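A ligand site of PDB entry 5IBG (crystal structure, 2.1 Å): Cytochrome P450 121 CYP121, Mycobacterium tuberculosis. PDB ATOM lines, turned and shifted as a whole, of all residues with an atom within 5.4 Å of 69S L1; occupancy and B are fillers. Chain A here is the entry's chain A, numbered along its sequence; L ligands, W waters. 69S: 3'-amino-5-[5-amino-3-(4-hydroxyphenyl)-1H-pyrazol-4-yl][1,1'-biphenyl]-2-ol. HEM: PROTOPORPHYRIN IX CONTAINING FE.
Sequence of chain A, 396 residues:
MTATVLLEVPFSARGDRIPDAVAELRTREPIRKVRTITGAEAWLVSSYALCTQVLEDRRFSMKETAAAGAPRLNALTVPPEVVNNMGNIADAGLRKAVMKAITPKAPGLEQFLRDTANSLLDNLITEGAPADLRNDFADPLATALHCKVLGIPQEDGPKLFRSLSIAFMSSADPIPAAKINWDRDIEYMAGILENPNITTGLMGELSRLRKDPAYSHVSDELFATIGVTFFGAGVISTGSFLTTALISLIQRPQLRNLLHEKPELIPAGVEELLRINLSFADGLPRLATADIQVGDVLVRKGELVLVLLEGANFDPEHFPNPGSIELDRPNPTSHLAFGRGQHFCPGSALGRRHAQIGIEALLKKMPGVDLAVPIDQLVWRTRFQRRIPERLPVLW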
ATOM      1  N   THR A  77     -15.832  15.512 -29.009  1.00  0.00           N
ATOM      2  CA  THR A  77     -15.543  15.448 -27.581  1.00  0.00           C
ATOM      3  C   THR A  77     -16.287  16.566 -26.851  1.00  0.00           C
ATOM      4  O   THR A  77     -16.070  16.800 -25.660  1.00  0.00           O
ATOM      5  CB  THR A  77     -14.038  15.567 -27.296  1.00  0.00           C
ATOM      6  OG1 THR A  77     -13.549  16.831 -27.779  1.00  0.00           O
ATOM      7  CG2 THR A  77     -13.280  14.445 -27.993  1.00  0.00           C
ATOM      8  N   VAL A  78     -17.141  17.261 -27.591  1.00  0.00           N
ATOM      9  CA  VAL A  78     -17.948  18.350 -27.057  1.00  0.00           C
ATOM     10  C   VAL A  78     -19.392  18.159 -27.509  1.00  0.00           C
ATOM     11  O   VAL A  78     -19.652  17.415 -28.457  1.00  0.00           O
ATOM     12  CB  VAL A  78     -17.426  19.732 -27.537  1.00  0.00           C
ATOM     13  CG1 VAL A  78     -16.067  20.038 -26.928  1.00  0.00           C
ATOM     14  CG2 VAL A  78     -17.367  19.780 -29.048  1.00  0.00           C
ATOM     15  N   VAL A  82     -21.379  23.138 -29.552  1.00  0.00           N
ATOM     16  CA  VAL A  82     -20.136  23.822 -29.233  1.00  0.00           C
ATOM     17  C   VAL A  82     -19.328  24.084 -30.511  1.00  0.00           C
ATOM     18  O   VAL A  82     -18.554  25.025 -30.580  1.00  0.00           O
ATOM     19  CB  VAL A  82     -19.289  23.005 -28.217  1.00  0.00           C
ATOM     20  CG1 VAL A  82     -17.982  23.713 -27.896  1.00  0.00           C
ATOM     21  CG2 VAL A  82     -20.091  22.764 -26.957  1.00  0.00           C
ATOM     22  N   LEU A 164      -7.863  18.538 -20.197  1.00  0.00           N
ATOM     23  CA  LEU A 164      -7.435  18.842 -21.558  1.00  0.00           C
ATOM     24  C   LEU A 164      -6.719  17.685 -22.265  1.00  0.00           C
ATOM     25  O   LEU A 164      -6.794  17.581 -23.494  1.00  0.00           O
ATOM     26  CB  LEU A 164      -6.548  20.089 -21.557  1.00  0.00           C
ATOM     27  CG  LEU A 164      -7.233  21.374 -21.080  1.00  0.00           C
ATOM     28  CD1 LEU A 164      -6.338  22.591 -21.334  1.00  0.00           C
ATOM     29  CD2 LEU A 164      -8.596  21.563 -21.717  1.00  0.00           C
ATOM     30  N   ALA A 167      -9.911  16.072 -23.425  1.00  0.00           N
ATOM     31  CA  ALA A 167     -10.792  16.972 -24.177  1.00  0.00           C
ATOM     32  C   ALA A 167     -10.308  17.216 -25.603  1.00  0.00           C
ATOM     33  O   ALA A 167     -11.132  17.358 -26.517  1.00  0.00           O
ATOM     34  CB  ALA A 167     -10.934  18.295 -23.442  1.00  0.00           C
ATOM     35  N   PHE A 168      -9.004  17.273 -25.814  1.00  0.00           N
ATOM     36  CA  PHE A 168      -8.470  17.555 -27.147  1.00  0.00           C
ATOM     37  C   PHE A 168      -7.839  16.341 -27.811  1.00  0.00           C
ATOM     38  O   PHE A 168      -6.977  16.475 -28.692  1.00  0.00           O
ATOM     39  CB  PHE A 168      -7.460  18.706 -27.091  1.00  0.00           C
ATOM     40  CG  PHE A 168      -8.109  20.057 -27.102  1.00  0.00           C
ATOM     41  CD1 PHE A 168      -8.479  20.689 -25.924  1.00  0.00           C
ATOM     42  CD2 PHE A 168      -8.394  20.687 -28.309  1.00  0.00           C
ATOM     43  CE1 PHE A 168      -9.087  21.927 -25.946  1.00  0.00           C
ATOM     44  CE2 PHE A 168      -9.001  21.925 -28.340  1.00  0.00           C
ATOM     45  CZ  PHE A 168      -9.352  22.545 -27.160  1.00  0.00           C
ATOM     46  N   TRP A 182     -16.536  17.284 -19.139  1.00  0.00           N
ATOM     47  CA  TRP A 182     -17.267  18.442 -19.645  1.00  0.00           C
ATOM     48  C   TRP A 182     -18.387  18.851 -18.701  1.00  0.00           C
ATOM     49  O   TRP A 182     -18.511  20.024 -18.359  1.00  0.00           O
ATOM     50  CB  TRP A 182     -17.835  18.146 -21.033  1.00  0.00           C
ATOM     51  CG  TRP A 182     -18.574  19.301 -21.621  1.00  0.00           C
ATOM     52  CD1 TRP A 182     -19.917  19.549 -21.529  1.00  0.00           C
ATOM     53  CD2 TRP A 182     -18.019  20.389 -22.369  1.00  0.00           C
ATOM     54  NE1 TRP A 182     -20.236  20.712 -22.187  1.00  0.00           N
ATOM     55  CE2 TRP A 182     -19.084  21.252 -22.707  1.00  0.00           C
ATOM     56  CE3 TRP A 182     -16.734  20.717 -22.788  1.00  0.00           C
ATOM     57  CZ2 TRP A 182     -18.899  22.414 -23.452  1.00  0.00           C
ATOM     58  CZ3 TRP A 182     -16.540  21.878 -23.522  1.00  0.00           C
ATOM     59  CH2 TRP A 182     -17.621  22.711 -23.844  1.00  0.00           C
ATOM     60  N   VAL A 228     -15.984  27.470 -20.351  1.00  0.00           N
ATOM     61  CA  VAL A 228     -15.263  26.209 -20.535  1.00  0.00           C
ATOM     62  C   VAL A 228     -14.528  26.189 -21.865  1.00  0.00           C
ATOM     63  O   VAL A 228     -13.355  25.803 -21.934  1.00  0.00           O
ATOM     64  CB  VAL A 228     -16.218  24.993 -20.474  1.00  0.00           C
ATOM     65  CG1 VAL A 228     -15.439  23.696 -20.661  1.00  0.00           C
ATOM     66  CG2 VAL A 228     -16.977  24.975 -19.151  1.00  0.00           C
ATOM     67  N   THR A 229     -15.204  26.622 -22.927  1.00  0.00           N
ATOM     68  CA  THR A 229     -14.639  26.600 -24.276  1.00  0.00           C
ATOM     69  C   THR A 229     -13.404  27.483 -24.403  1.00  0.00           C
ATOM     70  O   THR A 229     -12.369  27.045 -24.906  1.00  0.00           O
ATOM     71  CB  THR A 229     -15.674  27.035 -25.329  1.00  0.00           C
ATOM     72  OG1 THR A 229     -16.783  26.119 -25.315  1.00  0.00           O
ATOM     73  CG2 THR A 229     -15.049  27.040 -26.716  1.00  0.00           C
ATOM     74  N   PHE A 231     -11.460  28.751 -22.065  1.00  0.00           N
ATOM     75  CA  PHE A 231     -10.353  28.297 -21.225  1.00  0.00           C
ATOM     76  C   PHE A 231      -9.596  27.164 -21.913  1.00  0.00           C
ATOM     77  O   PHE A 231      -8.374  27.214 -22.067  1.00  0.00           O
ATOM     78  CB  PHE A 231     -10.830  27.835 -19.852  1.00  0.00           C
ATOM     79  CG  PHE A 231      -9.714  27.326 -18.974  1.00  0.00           C
ATOM     80  CD1 PHE A 231      -9.088  28.172 -18.079  1.00  0.00           C
ATOM     81  CD2 PHE A 231      -9.269  26.003 -19.067  1.00  0.00           C
ATOM     82  CE1 PHE A 231      -8.045  27.716 -17.280  1.00  0.00           C
ATOM     83  CE2 PHE A 231      -8.224  25.548 -18.278  1.00  0.00           C
ATOM     84  CZ  PHE A 231      -7.617  26.405 -17.385  1.00  0.00           C
ATOM     85  N   GLY A 232     -10.323  26.127 -22.319  1.00  0.00           N
ATOM     86  CA  GLY A 232      -9.712  24.939 -22.904  1.00  0.00           C
ATOM     87  C   GLY A 232      -9.008  25.224 -24.219  1.00  0.00           C
ATOM     88  O   GLY A 232      -7.846  24.839 -24.411  1.00  0.00           O
ATOM     89  N   ALA A 233      -9.705  25.888 -25.127  1.00  0.00           N
ATOM     90  CA  ALA A 233      -9.162  26.207 -26.436  1.00  0.00           C
ATOM     91  C   ALA A 233      -7.959  27.134 -26.332  1.00  0.00           C
ATOM     92  O   ALA A 233      -6.957  26.957 -27.027  1.00  0.00           O
ATOM     93  CB  ALA A 233     -10.245  26.833 -27.312  1.00  0.00           C
ATOM     94  N   GLY A 234      -8.064  28.141 -25.470  1.00  0.00           N
ATOM     95  CA  GLY A 234      -6.996  29.094 -25.275  1.00  0.00           C
ATOM     96  C   GLY A 234      -5.759  28.501 -24.625  1.00  0.00           C
ATOM     97  O   GLY A 234      -4.641  28.756 -25.067  1.00  0.00           O
ATOM     98  N   SER A 237      -4.010  25.912 -26.979  1.00  0.00           N
ATOM     99  CA  SER A 237      -3.443  26.475 -28.207  1.00  0.00           C
ATOM    100  C   SER A 237      -2.183  27.280 -27.907  1.00  0.00           C
ATOM    101  O   SER A 237      -1.190  27.166 -28.630  1.00  0.00           O
ATOM    102  CB  SER A 237      -4.474  27.336 -28.936  1.00  0.00           C
ATOM    103  OG  SER A 237      -5.578  26.567 -29.358  1.00  0.00           O
ATOM    104  N   PHE A 280      -0.610  22.088 -34.795  1.00  0.00           N
ATOM    105  CA  PHE A 280      -1.866  21.485 -35.233  1.00  0.00           C
ATOM    106  C   PHE A 280      -1.633  20.124 -35.863  1.00  0.00           C
ATOM    107  O   PHE A 280      -0.905  19.987 -36.856  1.00  0.00           O
ATOM    108  CB  PHE A 280      -2.596  22.409 -36.211  1.00  0.00           C
ATOM    109  CG  PHE A 280      -3.419  23.459 -35.540  1.00  0.00           C
ATOM    110  CD1 PHE A 280      -2.818  24.506 -34.859  1.00  0.00           C
ATOM    111  CD2 PHE A 280      -4.809  23.388 -35.559  1.00  0.00           C
ATOM    112  CE1 PHE A 280      -3.583  25.472 -34.225  1.00  0.00           C
ATOM    113  CE2 PHE A 280      -5.574  24.345 -34.934  1.00  0.00           C
ATOM    114  CZ  PHE A 280      -4.961  25.392 -34.262  1.00  0.00           C
ATOM    115  N   LEU A 284      -7.743  21.683 -40.657  1.00  0.00           N
ATOM    116  CA  LEU A 284      -8.995  22.287 -40.210  1.00  0.00           C
ATOM    117  C   LEU A 284     -10.144  21.673 -40.997  1.00  0.00           C
ATOM    118  O   LEU A 284     -10.128  21.662 -42.225  1.00  0.00           O
ATOM    119  CB  LEU A 284      -8.967  23.801 -40.390  1.00  0.00           C
ATOM    120  CG  LEU A 284      -7.843  24.554 -39.670  1.00  0.00           C
ATOM    121  CD1 LEU A 284      -8.008  26.056 -39.862  1.00  0.00           C
ATOM    122  CD2 LEU A 284      -7.797  24.196 -38.191  1.00  0.00           C
ATOM    123  N   CYS A 345      -9.080  33.247 -35.786  1.00  0.00           N
ATOM    124  CA  CYS A 345      -8.922  33.143 -34.332  1.00  0.00           C
ATOM    125  C   CYS A 345      -9.141  34.475 -33.620  1.00  0.00           C
ATOM    126  O   CYS A 345      -8.410  35.434 -33.849  1.00  0.00           O
ATOM    127  CB  CYS A 345      -7.539  32.583 -33.991  1.00  0.00           C
ATOM    128  SG  CYS A 345      -7.327  32.336 -32.212  1.00  0.00           S
ATOM    129  N   GLN A 385      -5.190  16.403 -30.821  1.00  0.00           N
ATOM    130  CA  GLN A 385      -5.450  17.492 -31.759  1.00  0.00           C
ATOM    131  C   GLN A 385      -4.272  18.477 -31.838  1.00  0.00           C
ATOM    132  O   GLN A 385      -4.231  19.341 -32.709  1.00  0.00           O
ATOM    133  CB  GLN A 385      -6.736  18.236 -31.381  1.00  0.00           C
ATOM    134  CG  GLN A 385      -7.993  17.388 -31.540  1.00  0.00           C
ATOM    135  CD  GLN A 385      -9.264  18.119 -31.139  1.00  0.00           C
ATOM    136  OE1 GLN A 385     -10.111  17.565 -30.436  1.00  0.00           O
ATOM    137  NE2 GLN A 385      -9.396  19.366 -31.577  1.00  0.00           N
ATOM    138  N   ARG A 386      -3.327  18.324 -30.925  1.00  0.00           N
ATOM    139  CA  ARG A 386      -2.084  19.090 -30.987  1.00  0.00           C
ATOM    140  C   ARG A 386      -0.871  18.164 -31.034  1.00  0.00           C
ATOM    141  O   ARG A 386      -0.911  17.057 -30.515  1.00  0.00           O
ATOM    142  CB  ARG A 386      -1.943  20.046 -29.791  1.00  0.00           C
ATOM    143  CG  ARG A 386      -2.973  21.166 -29.740  1.00  0.00           C
ATOM    144  CD  ARG A 386      -2.852  22.118 -30.917  1.00  0.00           C
ATOM    145  NE  ARG A 386      -3.821  23.209 -30.827  1.00  0.00           N
ATOM    146  CZ  ARG A 386      -5.092  23.098 -31.224  1.00  0.00           C
ATOM    147  NH1 ARG A 386      -5.917  24.142 -31.103  1.00  0.00           N
ATOM    148  NH2 ARG A 386      -5.538  21.962 -31.732  1.00  0.00           N
HETATM  149  C2  69S L   1     -12.655  21.544 -26.682  1.00  0.00           C
HETATM  150  C3  69S L   1     -12.499  22.901 -26.443  1.00  0.00           C
HETATM  151  C4  69S L   1     -12.577  23.395 -25.143  1.00  0.00           C
HETATM  152  C5  69S L   1     -12.801  22.533 -24.090  1.00  0.00           C
HETATM  153  C6  69S L   1     -12.949  21.175 -24.317  1.00  0.00           C
HETATM  154  C7  69S L   1     -12.861  20.680 -25.616  1.00  0.00           C
HETATM  155  C20 69S L   1     -11.617  23.711 -30.306  1.00  0.00           C
HETATM  156  C21 69S L   1     -10.430  25.567 -31.301  1.00  0.00           C
HETATM  157  C24 69S L   1      -8.137  26.529 -32.482  1.00  0.00           C
HETATM  158  C25 69S L   1      -8.910  25.608 -33.153  1.00  0.00           C
HETATM  159  C9  69S L   1     -12.544  20.942 -28.066  1.00  0.00           C
HETATM  160  C10 69S L   1     -12.597  21.565 -29.325  1.00  0.00           C
HETATM  161  C11 69S L   1     -12.401  20.598 -30.281  1.00  0.00           C
HETATM  162  C15 69S L   1     -12.785  23.040 -29.645  1.00  0.00           C
HETATM  163  C16 69S L   1     -13.905  23.747 -29.373  1.00  0.00           C
HETATM  164  C17 69S L   1     -13.953  25.212 -29.741  1.00  0.00           C
HETATM  165  C19 69S L   1     -11.668  25.003 -30.645  1.00  0.00           C
HETATM  166  C22 69S L   1      -9.647  26.486 -30.629  1.00  0.00           C
HETATM  167  C23 69S L   1      -8.509  26.974 -31.225  1.00  0.00           C
HETATM  168  N1  69S L   1      -7.718  27.930 -30.518  1.00  0.00           N
HETATM  169  O27 69S L   1     -12.948  27.181 -30.679  1.00  0.00           O
HETATM  170  O8  69S L   1     -12.883  23.027 -22.770  1.00  0.00           O
HETATM  171  N12 69S L   1     -12.240  19.380 -29.632  1.00  0.00           N
HETATM  172  N13 69S L   1     -12.317  19.608 -28.268  1.00  0.00           N
HETATM  173  N14 69S L   1     -12.384  20.793 -31.688  1.00  0.00           N
HETATM  174  C18 69S L   1     -12.905  25.819 -30.335  1.00  0.00           C
HETATM  175  C26 69S L   1     -10.060  25.111 -32.549  1.00  0.00           C
HETATM  176  CHA HEM L   2     -10.089  29.625 -33.850  1.00  0.00           C
HETATM  177  CHB HEM L   2      -5.301  28.913 -33.689  1.00  0.00           C
HETATM  178  CHC HEM L   2      -5.147  31.019 -29.335  1.00  0.00           C
HETATM  179  CHD HEM L   2     -10.004  30.890 -29.126  1.00  0.00           C
HETATM  180  C1A HEM L   2      -8.812  29.294 -34.213  1.00  0.00           C
HETATM  181  C2A HEM L   2      -8.389  28.786 -35.507  1.00  0.00           C
HETATM  182  C3A HEM L   2      -7.073  28.589 -35.458  1.00  0.00           C
HETATM  183  C4A HEM L   2      -6.608  28.971 -34.133  1.00  0.00           C
HETATM  184  CMA HEM L   2      -6.188  28.057 -36.602  1.00  0.00           C
HETATM  185  CAA HEM L   2      -9.297  28.509 -36.738  1.00  0.00           C
HETATM  186  CBA HEM L   2     -10.083  27.209 -36.582  1.00  0.00           C
HETATM  187  CGA HEM L   2     -10.911  26.924 -37.810  1.00  0.00           C
HETATM  188  O1A HEM L   2     -11.026  27.804 -38.707  1.00  0.00           O
HETATM  189  O2A HEM L   2     -11.472  25.805 -37.909  1.00  0.00           O
HETATM  190  C1B HEM L   2      -4.823  29.467 -32.514  1.00  0.00           C
HETATM  191  C2B HEM L   2      -3.431  29.609 -32.144  1.00  0.00           C
HETATM  192  C3B HEM L   2      -3.385  30.190 -30.929  1.00  0.00           C
HETATM  193  C4B HEM L   2      -4.751  30.435 -30.516  1.00  0.00           C
HETATM  194  CMB HEM L   2      -2.254  29.140 -33.042  1.00  0.00           C
HETATM  195  CAB HEM L   2      -2.161  30.588 -30.053  1.00  0.00           C
HETATM  196  CBB HEM L   2      -0.887  30.543 -30.458  1.00  0.00           C
HETATM  197  C1C HEM L   2      -6.450  31.197 -28.915  1.00  0.00           C
HETATM  198  C2C HEM L   2      -6.858  31.849 -27.681  1.00  0.00           C
HETATM  199  C3C HEM L   2      -8.205  31.819 -27.628  1.00  0.00           C
HETATM  200  C4C HEM L   2      -8.675  31.134 -28.812  1.00  0.00           C
HETATM  201  CMC HEM L   2      -5.857  32.458 -26.676  1.00  0.00           C
HETATM  202  CAC HEM L   2      -9.172  32.353 -26.538  1.00  0.00           C
HETATM  203  CBC HEM L   2      -8.791  32.908 -25.389  1.00  0.00           C
HETATM  204  C1D HEM L   2     -10.501  30.545 -30.362  1.00  0.00           C
HETATM  205  C2D HEM L   2     -11.899  30.400 -30.692  1.00  0.00           C
HETATM  206  C3D HEM L   2     -11.913  29.999 -32.175  1.00  0.00           C
HETATM  207  C4D HEM L   2     -10.528  29.944 -32.582  1.00  0.00           C
HETATM  208  CMD HEM L   2     -13.119  30.599 -29.769  1.00  0.00           C
HETATM  209  CAD HEM L   2     -13.143  29.714 -33.065  1.00  0.00           C
HETATM  210  CBD HEM L   2     -13.457  30.978 -33.868  1.00  0.00           C
HETATM  211  CGD HEM L   2     -14.690  30.749 -34.704  1.00  0.00           C
HETATM  212  O1D HEM L   2     -15.154  31.721 -35.339  1.00  0.00           O
HETATM  213  O2D HEM L   2     -15.208  29.599 -34.717  1.00  0.00           O
HETATM  214  NA  HEM L   2      -7.691  29.404 -33.394  1.00  0.00           N
HETATM  215  NB  HEM L   2      -5.597  29.979 -31.494  1.00  0.00           N
HETATM  216  NC  HEM L   2      -7.590  30.773 -29.575  1.00  0.00           N
HETATM  217  ND  HEM L   2      -9.734  30.274 -31.490  1.00  0.00           N
HETATM  218 FE   HEM L   2      -7.670  30.204 -31.508  1.00  0.00          FE
HETATM  219  O   HOH W   1     -12.968  25.919 -33.806  1.00  0.00           O
HETATM  220  O   HOH W   2     -15.504  28.040 -30.255  1.00  0.00           O
HETATM  221  O   HOH W   3     -14.694  19.975 -32.239  1.00  0.00           O
HETATM  222  O   HOH W   4     -14.192  18.366 -24.411  1.00  0.00           O
HETATM  223  O   HOH W   5     -12.646  23.079 -33.950  1.00  0.00           O
HETATM  224  O   HOH W   6     -14.342  17.633 -30.504  1.00  0.00           O
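The backbone carbonyl oxygen (O) of Ala 167 sits close to a nitrogen (N13) of 69S L1 (3.1 Å).
OG1 of Thr 77 lies within hydrogen-bond range of N13 of 69S L1.
The side-chain amide oxygen (OE1) of Gln 385 lies within hydrogen-bond range of a nitrogen (N12) of 69S L1, 2.9 Å away.
The side-chain sulfur (SG) of Cys 345 binds an iron atom (FE) of HEM L2 (2.3 Å).
The side-chain hydroxyl of Ser 237 sits close to a nitrogen (N1) of 69S L1.
An oxygen (O8) of 69S L1 sits at hydrogen-bond distance from the backbone carbonyl oxygen of Val 228, 2.9 Å away.
A nitrogen (N1) of 69S L1 is bound to an iron atom (FE) of HEM L2.
The side-chain hydroxyl of Thr 77 is in hydrogen-bond range of the backbone carbonyl oxygen of Ala 167 (2.8 Å).
The side-chain hydroxyl (OG) of Ser 237 sits at hydrogen-bond distance from the backbone carbonyl oxygen (O) of Ala 233, 2.7 Å away.
The backbone NH (N) of Gln 385 sits at hydrogen-bond distance from the backbone carbonyl oxygen (O) of Phe 168 (2.8 Å).
The guanidinium group (NH1) of Arg 386 lies within hydrogen-bond range of the side-chain hydroxyl (OG) of Ser 237 (3.0 Å).
Val 78 touches 69S L1.
Phe 168 touches 69S L1.
CZ3 of Trp 182 touches C6 of 69S L1, 3.7 Å away.
O of Thr 229 touches C4 of 69S L1 (3.7 Å).
Gly 232 touches 69S L1 (CA to O8, 3.7 Å).
Ala 233 touches 69S L1.
CZ of Phe 280 touches C24 of 69S L1, 3.8 Å away.
NH1 of Arg 386 touches C24 of 69S L1 (3.5 Å).
Of the 19 residues printed, 13 come within 4 Å of 69S L1.
Water W6 lies within hydrogen-bond range of N12 of 69S L1 (2.9 Å) and OG1 of Thr 77 (2.9 Å).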
